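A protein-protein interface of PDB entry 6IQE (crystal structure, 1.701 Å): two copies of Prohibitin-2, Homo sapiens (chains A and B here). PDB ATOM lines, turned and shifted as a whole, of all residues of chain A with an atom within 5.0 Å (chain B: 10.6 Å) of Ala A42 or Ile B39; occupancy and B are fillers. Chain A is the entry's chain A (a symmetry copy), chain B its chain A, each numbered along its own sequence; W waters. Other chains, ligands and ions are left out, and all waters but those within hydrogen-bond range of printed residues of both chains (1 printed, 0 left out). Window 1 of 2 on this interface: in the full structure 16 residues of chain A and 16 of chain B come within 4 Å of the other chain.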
ATOM      1  N   LYS A  38      20.428 -25.930  31.210  1.00  0.00           N
ATOM      2  CA  LYS A  38      21.120 -26.455  30.027  1.00  0.00           C
ATOM      3  C   LYS A  38      20.293 -26.265  28.751  1.00  0.00           C
ATOM      4  O   LYS A  38      20.838 -25.999  27.675  1.00  0.00           O
ATOM      5  CB  LYS A  38      21.451 -27.937  30.213  1.00  0.00           C
ATOM      6  CG  LYS A  38      22.644 -28.181  31.132  1.00  0.00           C
ATOM      7  CD  LYS A  38      22.937 -29.671  31.268  1.00  0.00           C
ATOM      8  CE  LYS A  38      24.104 -29.928  32.208  1.00  0.00           C
ATOM      9  NZ  LYS A  38      25.348 -29.251  31.738  1.00  0.00           N
ATOM     10  N   ILE A  39      18.980 -26.400  28.872  1.00  0.00           N
ATOM     11  CA  ILE A  39      18.093 -26.136  27.748  1.00  0.00           C
ATOM     12  C   ILE A  39      18.139 -24.655  27.341  1.00  0.00           C
ATOM     13  O   ILE A  39      18.218 -24.326  26.154  1.00  0.00           O
ATOM     14  CB  ILE A  39      16.639 -26.549  28.076  1.00  0.00           C
ATOM     15  CG1 ILE A  39      16.562 -28.069  28.331  1.00  0.00           C
ATOM     16  CG2 ILE A  39      15.705 -26.149  26.940  1.00  0.00           C
ATOM     17  CD1 ILE A  39      15.228 -28.507  28.941  1.00  0.00           C
ATOM     18  N   VAL A  40      18.112 -23.761  28.326  1.00  0.00           N
ATOM     19  CA  VAL A  40      18.171 -22.323  28.030  1.00  0.00           C
ATOM     20  C   VAL A  40      19.488 -21.928  27.329  1.00  0.00           C
ATOM     21  O   VAL A  40      19.503 -21.166  26.342  1.00  0.00           O
ATOM     22  CB  VAL A  40      17.999 -21.486  29.313  1.00  0.00           C
ATOM     23  CG1 VAL A  40      18.366 -20.029  29.059  1.00  0.00           C
ATOM     24  CG2 VAL A  40      16.575 -21.593  29.825  1.00  0.00           C
ATOM     25  N   GLN A  41      20.586 -22.470  27.833  1.00  0.00           N
ATOM     26  CA  GLN A  41      21.907 -22.246  27.257  1.00  0.00           C
ATOM     27  C   GLN A  41      21.981 -22.722  25.804  1.00  0.00           C
ATOM     28  O   GLN A  41      22.392 -21.979  24.913  1.00  0.00           O
ATOM     29  CB  GLN A  41      22.963 -22.958  28.092  1.00  0.00           C
ATOM     30  CG  GLN A  41      23.212 -22.315  29.440  1.00  0.00           C
ATOM     31  CD  GLN A  41      24.110 -23.172  30.318  1.00  0.00           C
ATOM     32  OE1 GLN A  41      24.429 -24.305  29.973  1.00  0.00           O
ATOM     33  NE2 GLN A  41      24.495 -22.640  31.469  1.00  0.00           N
ATOM     34  N   ALA A  42      21.588 -23.973  25.563  1.00  0.00           N
ATOM     35  CA  ALA A  42      21.631 -24.540  24.214  1.00  0.00           C
ATOM     36  C   ALA A  42      20.652 -23.908  23.220  1.00  0.00           C
ATOM     37  O   ALA A  42      20.994 -23.718  22.049  1.00  0.00           O
ATOM     38  CB  ALA A  42      21.388 -26.045  24.275  1.00  0.00           C
ATOM     39  N   GLU A  43      19.434 -23.617  23.655  1.00  0.00           N
ATOM     40  CA  GLU A  43      18.494 -22.917  22.789  1.00  0.00           C
ATOM     41  C   GLU A  43      19.070 -21.552  22.402  1.00  0.00           C
ATOM     42  O   GLU A  43      18.916 -21.087  21.266  1.00  0.00           O
ATOM     43  CB  GLU A  43      17.138 -22.764  23.487  1.00  0.00           C
ATOM     44  CG  GLU A  43      16.356 -24.061  23.537  1.00  0.00           C
ATOM     45  CD  GLU A  43      15.050 -23.935  24.297  1.00  0.00           C
ATOM     46  OE1 GLU A  43      14.888 -22.948  25.055  1.00  0.00           O
ATOM     47  OE2 GLU A  43      14.197 -24.839  24.145  1.00  0.00           O
ATOM     48  N   GLY A  44      19.730 -20.913  23.356  1.00  0.00           N
ATOM     49  CA  GLY A  44      20.393 -19.653  23.084  1.00  0.00           C
ATOM     50  C   GLY A  44      21.488 -19.727  22.034  1.00  0.00           C
ATOM     51  O   GLY A  44      21.515 -18.949  21.069  1.00  0.00           O
ATOM     52  N   GLU A  45      22.388 -20.687  22.188  1.00  0.00           N
ATOM     53  CA  GLU A  45      23.467 -20.842  21.222  1.00  0.00           C
ATOM     54  C   GLU A  45      22.935 -21.373  19.886  1.00  0.00           C
ATOM     55  O   GLU A  45      23.427 -20.973  18.818  1.00  0.00           O
ATOM     56  CB  GLU A  45      24.572 -21.723  21.813  1.00  0.00           C
ATOM     57  CG  GLU A  45      25.376 -20.945  22.877  1.00  0.00           C
ATOM     58  CD  GLU A  45      26.534 -21.710  23.463  1.00  0.00           C
ATOM     59  OE1 GLU A  45      26.484 -22.953  23.483  1.00  0.00           O
ATOM     60  OE2 GLU A  45      27.497 -21.060  23.914  1.00  0.00           O
ATOM     61  N   ALA A  46      21.916 -22.235  19.930  1.00  0.00           N
ATOM     62  CA  ALA A  46      21.256 -22.660  18.694  1.00  0.00           C
ATOM     63  C   ALA A  46      20.701 -21.467  17.926  1.00  0.00           C
ATOM     64  O   ALA A  46      20.858 -21.392  16.713  1.00  0.00           O
ATOM     65  CB  ALA A  46      20.133 -23.690  18.980  1.00  0.00           C
ATOM     66  N   GLU A  47      20.109 -20.502  18.635  1.00  0.00           N
ATOM     67  CA  GLU A  47      19.522 -19.342  17.966  1.00  0.00           C
ATOM     68  C   GLU A  47      20.615 -18.431  17.375  1.00  0.00           C
ATOM     69  O   GLU A  47      20.476 -17.923  16.261  1.00  0.00           O
ATOM     70  CB  GLU A  47      18.633 -18.555  18.936  1.00  0.00           C
ATOM     71  CG  GLU A  47      18.060 -17.234  18.361  1.00  0.00           C
ATOM     72  CD  GLU A  47      17.076 -17.452  17.214  1.00  0.00           C
ATOM     73  OE1 GLU A  47      16.586 -18.585  17.032  1.00  0.00           O
ATOM     74  OE2 GLU A  47      16.790 -16.484  16.483  1.00  0.00           O
ATOM     75  N   LYS B  30      27.308 -27.489  11.749  1.00  0.00           N
ATOM     76  CA  LYS B  30      27.881 -28.365  12.770  1.00  0.00           C
ATOM     77  C   LYS B  30      27.499 -27.878  14.176  1.00  0.00           C
ATOM     78  O   LYS B  30      27.072 -28.665  15.017  1.00  0.00           O
ATOM     79  CB  LYS B  30      29.400 -28.439  12.611  1.00  0.00           C
ATOM     80  CG  LYS B  30      30.131 -29.294  13.641  1.00  0.00           C
ATOM     81  CD  LYS B  30      31.570 -29.521  13.196  1.00  0.00           C
ATOM     82  CE  LYS B  30      32.513 -29.753  14.354  1.00  0.00           C
ATOM     83  NZ  LYS B  30      32.162 -30.953  15.131  1.00  0.00           N
ATOM     84  N   ALA B  31      27.635 -26.577  14.413  1.00  0.00           N
ATOM     85  CA  ALA B  31      27.314 -25.982  15.716  1.00  0.00           C
ATOM     86  C   ALA B  31      25.823 -26.086  16.010  1.00  0.00           C
ATOM     87  O   ALA B  31      25.423 -26.405  17.138  1.00  0.00           O
ATOM     88  CB  ALA B  31      27.770 -24.524  15.769  1.00  0.00           C
ATOM     89  N   LYS B  32      25.003 -25.830  14.992  1.00  0.00           N
ATOM     90  CA  LYS B  32      23.551 -25.950  15.107  1.00  0.00           C
ATOM     91  C   LYS B  32      23.151 -27.345  15.564  1.00  0.00           C
ATOM     92  O   LYS B  32      22.360 -27.524  16.484  1.00  0.00           O
ATOM     93  CB  LYS B  32      22.871 -25.660  13.767  1.00  0.00           C
ATOM     94  CG  LYS B  32      22.599 -24.207  13.476  1.00  0.00           C
ATOM     95  CD  LYS B  32      21.434 -24.100  12.495  1.00  0.00           C
ATOM     96  CE  LYS B  32      21.798 -23.301  11.274  1.00  0.00           C
ATOM     97  NZ  LYS B  32      20.592 -23.130  10.417  1.00  0.00           N
ATOM     98  N   GLN B  33      23.717 -28.336  14.898  1.00  0.00           N
ATOM     99  CA  GLN B  33      23.379 -29.723  15.155  1.00  0.00           C
ATOM    100  C   GLN B  33      23.839 -30.181  16.550  1.00  0.00           C
ATOM    101  O   GLN B  33      23.115 -30.904  17.244  1.00  0.00           O
ATOM    102  CB  GLN B  33      23.966 -30.578  14.034  1.00  0.00           C
ATOM    103  CG  GLN B  33      24.443 -31.940  14.414  1.00  0.00           C
ATOM    104  CD  GLN B  33      25.789 -32.259  13.765  1.00  0.00           C
ATOM    105  OE1 GLN B  33      25.863 -32.533  12.559  1.00  0.00           O
ATOM    106  NE2 GLN B  33      26.864 -32.203  14.557  1.00  0.00           N
ATOM    107  N   GLU B  34      25.014 -29.737  16.976  1.00  0.00           N
ATOM    108  CA  GLU B  34      25.491 -30.038  18.323  1.00  0.00           C
ATOM    109  C   GLU B  34      24.573 -29.410  19.387  1.00  0.00           C
ATOM    110  O   GLU B  34      24.294 -30.018  20.424  1.00  0.00           O
ATOM    111  CB  GLU B  34      26.930 -29.556  18.511  1.00  0.00           C
ATOM    112  CG  GLU B  34      27.944 -30.310  17.646  1.00  0.00           C
ATOM    113  CD  GLU B  34      29.351 -29.736  17.728  1.00  0.00           C
ATOM    114  OE1 GLU B  34      29.569 -28.765  18.486  1.00  0.00           O
ATOM    115  OE2 GLU B  34      30.243 -30.262  17.023  1.00  0.00           O
ATOM    116  N   GLN B  35      24.103 -28.194  19.151  1.00  0.00           N
ATOM    117  CA  GLN B  35      23.237 -27.587  20.147  1.00  0.00           C
ATOM    118  C   GLN B  35      21.868 -28.263  20.160  1.00  0.00           C
ATOM    119  O   GLN B  35      21.279 -28.440  21.230  1.00  0.00           O
ATOM    120  CB  GLN B  35      23.118 -26.079  19.925  1.00  0.00           C
ATOM    121  CG  GLN B  35      24.461 -25.369  20.121  1.00  0.00           C
ATOM    122  CD  GLN B  35      25.110 -25.673  21.471  1.00  0.00           C
ATOM    123  OE1 GLN B  35      26.261 -26.123  21.537  1.00  0.00           O
ATOM    124  NE2 GLN B  35      24.382 -25.411  22.552  1.00  0.00           N
ATOM    125  N   ARG B  36      21.380 -28.687  18.994  1.00  0.00           N
ATOM    126  CA  ARG B  36      20.111 -29.412  18.922  1.00  0.00           C
ATOM    127  C   ARG B  36      20.204 -30.697  19.729  1.00  0.00           C
ATOM    128  O   ARG B  36      19.273 -31.062  20.442  1.00  0.00           O
ATOM    129  CB  ARG B  36      19.724 -29.734  17.472  1.00  0.00           C
ATOM    130  CG  ARG B  36      19.198 -28.544  16.669  1.00  0.00           C
ATOM    131  CD  ARG B  36      18.585 -28.988  15.336  1.00  0.00           C
ATOM    132  NE  ARG B  36      19.566 -29.614  14.452  1.00  0.00           N
ATOM    133  CZ  ARG B  36      20.021 -29.065  13.330  1.00  0.00           C
ATOM    134  NH1 ARG B  36      19.577 -27.877  12.941  1.00  0.00           N
ATOM    135  NH2 ARG B  36      20.914 -29.707  12.595  1.00  0.00           N
ATOM    136  N   GLN B  37      21.332 -31.383  19.607  1.00  0.00           N
ATOM    137  CA  GLN B  37      21.543 -32.606  20.373  1.00  0.00           C
ATOM    138  C   GLN B  37      21.597 -32.320  21.873  1.00  0.00           C
ATOM    139  O   GLN B  37      21.075 -33.105  22.674  1.00  0.00           O
ATOM    140  CB  GLN B  37      22.815 -33.314  19.903  1.00  0.00           C
ATOM    141  CG  GLN B  37      23.143 -34.624  20.615  1.00  0.00           C
ATOM    142  CD  GLN B  37      22.052 -35.693  20.495  1.00  0.00           C
ATOM    143  OE1 GLN B  37      21.144 -35.602  19.659  1.00  0.00           O
ATOM    144  NE2 GLN B  37      22.166 -36.734  21.320  1.00  0.00           N
ATOM    145  N   LYS B  38      22.201 -31.196  22.266  1.00  0.00           N
ATOM    146  CA  LYS B  38      22.239 -30.829  23.686  1.00  0.00           C
ATOM    147  C   LYS B  38      20.839 -30.540  24.239  1.00  0.00           C
ATOM    148  O   LYS B  38      20.535 -30.858  25.393  1.00  0.00           O
ATOM    149  CB  LYS B  38      23.141 -29.612  23.902  1.00  0.00           C
ATOM    150  CG  LYS B  38      24.630 -29.944  23.854  1.00  0.00           C
ATOM    151  CD  LYS B  38      25.478 -28.700  24.088  1.00  0.00           C
ATOM    152  CE  LYS B  38      26.964 -29.013  24.010  1.00  0.00           C
ATOM    153  NZ  LYS B  38      27.362 -30.043  25.014  1.00  0.00           N
ATOM    154  N   ILE B  39      19.992 -29.941  23.416  1.00  0.00           N
ATOM    155  CA  ILE B  39      18.606 -29.715  23.801  1.00  0.00           C
ATOM    156  C   ILE B  39      17.857 -31.046  23.981  1.00  0.00           C
ATOM    157  O   ILE B  39      17.122 -31.234  24.954  1.00  0.00           O
ATOM    158  CB  ILE B  39      17.874 -28.833  22.763  1.00  0.00           C
ATOM    159  CG1 ILE B  39      18.528 -27.437  22.696  1.00  0.00           C
ATOM    160  CG2 ILE B  39      16.396 -28.715  23.116  1.00  0.00           C
ATOM    161  CD1 ILE B  39      18.054 -26.611  21.498  1.00  0.00           C
ATOM    162  N   VAL B  40      18.059 -31.978  23.052  1.00  0.00           N
ATOM    163  CA  VAL B  40      17.398 -33.286  23.153  1.00  0.00           C
ATOM    164  C   VAL B  40      17.825 -34.056  24.421  1.00  0.00           C
ATOM    165  O   VAL B  40      16.996 -34.643  25.143  1.00  0.00           O
ATOM    166  CB  VAL B  40      17.684 -34.147  21.906  1.00  0.00           C
ATOM    167  CG1 VAL B  40      17.266 -35.594  22.144  1.00  0.00           C
ATOM    168  CG2 VAL B  40      16.963 -33.579  20.698  1.00  0.00           C
ATOM    169  N   GLN B  41      19.121 -34.028  24.694  1.00  0.00           N
ATOM    170  CA  GLN B  41      19.685 -34.658  25.882  1.00  0.00           C
ATOM    171  C   GLN B  41      19.097 -34.071  27.168  1.00  0.00           C
ATOM    172  O   GLN B  41      18.621 -34.800  28.038  1.00  0.00           O
ATOM    173  CB  GLN B  41      21.200 -34.498  25.882  1.00  0.00           C
ATOM    174  CG  GLN B  41      21.904 -35.346  24.845  1.00  0.00           C
ATOM    175  CD  GLN B  41      23.380 -35.000  24.738  1.00  0.00           C
ATOM    176  OE1 GLN B  41      23.843 -34.035  25.336  1.00  0.00           O
ATOM    177  NE2 GLN B  41      24.114 -35.772  23.950  1.00  0.00           N
ATOM    178  N   ALA B  42      19.140 -32.745  27.295  1.00  0.00           N
ATOM    179  CA  ALA B  42      18.622 -32.075  28.490  1.00  0.00           C
ATOM    180  C   ALA B  42      17.105 -32.171  28.673  1.00  0.00           C
ATOM    181  O   ALA B  42      16.624 -32.332  29.799  1.00  0.00           O
ATOM    182  CB  ALA B  42      19.039 -30.608  28.486  1.00  0.00           C
ATOM    183  N   GLU B  43      16.344 -32.036  27.596  1.00  0.00           N
ATOM    184  CA  GLU B  43      14.902 -32.225  27.687  1.00  0.00           C
ATOM    185  C   GLU B  43      14.598 -33.648  28.163  1.00  0.00           C
ATOM    186  O   GLU B  43      13.670 -33.881  28.947  1.00  0.00           O
ATOM    187  CB  GLU B  43      14.240 -31.944  26.334  1.00  0.00           C
ATOM    188  CG  GLU B  43      14.176 -30.465  26.009  1.00  0.00           C
ATOM    189  CD  GLU B  43      13.596 -30.186  24.637  1.00  0.00           C
ATOM    190  OE1 GLU B  43      13.536 -31.125  23.806  1.00  0.00           O
ATOM    191  OE2 GLU B  43      13.219 -29.017  24.389  1.00  0.00           O
ATOM    192  N   GLY B  44      15.383 -34.598  27.678  1.00  0.00           N
ATOM    193  CA  GLY B  44      15.247 -35.971  28.122  1.00  0.00           C
ATOM    194  C   GLY B  44      15.490 -36.185  29.606  1.00  0.00           C
ATOM    195  O   GLY B  44      14.675 -36.793  30.315  1.00  0.00           O
ATOM    196  N   GLU B  45      16.597 -35.656  30.104  1.00  0.00           N
ATOM    197  CA  GLU B  45      16.905 -35.799  31.521  1.00  0.00           C
ATOM    198  C   GLU B  45      15.957 -34.950  32.376  1.00  0.00           C
ATOM    199  O   GLU B  45      15.568 -35.372  33.477  1.00  0.00           O
ATOM    200  CB  GLU B  45      18.381 -35.473  31.768  1.00  0.00           C
ATOM    201  CG  GLU B  45      19.283 -36.618  31.259  1.00  0.00           C
ATOM    202  CD  GLU B  45      20.752 -36.417  31.526  1.00  0.00           C
ATOM    203  OE1 GLU B  45      21.191 -35.259  31.633  1.00  0.00           O
ATOM    204  OE2 GLU B  45      21.473 -37.430  31.622  1.00  0.00           O
ATOM    205  N   ALA B  46      15.554 -33.782  31.870  1.00  0.00           N
ATOM    206  CA  ALA B  46      14.530 -32.995  32.558  1.00  0.00           C
ATOM    207  C   ALA B  46      13.242 -33.792  32.728  1.00  0.00           C
ATOM    208  O   ALA B  46      12.645 -33.773  33.798  1.00  0.00           O
ATOM    209  CB  ALA B  46      14.248 -31.663  31.817  1.00  0.00           C
ATOM    210  N   GLU B  47      12.846 -34.545  31.698  1.00  0.00           N
ATOM    211  CA  GLU B  47      11.603 -35.312  31.773  1.00  0.00           C
ATOM    212  C   GLU B  47      11.734 -36.485  32.762  1.00  0.00           C
ATOM    213  O   GLU B  47      10.814 -36.766  33.531  1.00  0.00           O
ATOM    214  CB  GLU B  47      11.202 -35.821  30.383  1.00  0.00           C
ATOM    215  CG  GLU B  47       9.962 -36.752  30.369  1.00  0.00           C
ATOM    216  CD  GLU B  47       8.672 -36.046  30.778  1.00  0.00           C
ATOM    217  OE1 GLU B  47       8.631 -34.798  30.787  1.00  0.00           O
ATOM    218  OE2 GLU B  47       7.687 -36.741  31.096  1.00  0.00           O
HETATM  219  O   HOH W   1      25.036 -25.285  25.214  1.00  0.00           O
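Of the printed residues of chain B, Ala A42 touches Gln B35, Lys B38 and Ile B39. Ile B39 touches just these residues of chain A: Ala A42 (3.6 Å) and Glu A43 (3.7 Å). Ile A39 touches just these residues of chain B: Ala B42 and Glu B43. Of chain B, only Ile B39 comes within 4 Å of Glu A43. No residue of chain B comes within 4 Å of Gly A44. Of the printed residues of chain A, Glu B43 touches Ile A39 (3.7 Å). Of the printed residues of chain B, Glu A45 touches Gln B35. Printed residues of chain B within 4 Å of Ala A46: Gln B35 (3.9 Å). Of the printed residues of chain A, Gln B35 touches Ala A42, Glu A45 and Ala A46. Gly B44 touches none of the printed residues of chain A.
Lys A38 touches Ala B42, and with the chains exchanged Ala A42 touches Lys B38. Ile A39 touches Ala B42, and with the chains exchanged Ala A42 touches Ile B39. Ile A39 touches Glu B43, and with the chains exchanged Glu A43 touches Ile B39. Positions printed for both chains: 38, 39, 40, 41, 42, 43, 44, 45, 46 and 47.
Water W1 bridges NE2 of Gln B35 (2.7 Å) and OE1 of Glu A45 (3.2 Å).
Printed residues of chain B that touch a printed residue of chain A: Gln B35, Lys B38, Ile B39, Ala B42 and Glu B43. Hydrophobic or aromatic side chains of chain B within 4 Å of the printed part of chain A: Ile B39 and Ala B42. Among the printed residues, 9 pairs touch across the chains.
Among the printed residues, pairs that only touch across the chains: Ala A42 with Gln B35 (3.3 Å), Ile A39 with Ala B42 (3.6 Å), Ala A42 with Ile B39 (3.6 Å), Ile A39 with Glu B43 (3.7 Å), Glu A43 with Ile B39 (3.7 Å), Ala A46 with Gln B35 (3.9 Å), Lys A38 with Ala B42 (3.99 Å) and Ala A42 with Lys B38 (3.99 Å).
The side-chain amide nitrogen (NE2) of Gln B35 lies within hydrogen-bond range of the side-chain carboxylate (OE1) of Glu A45 (3.4 Å).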
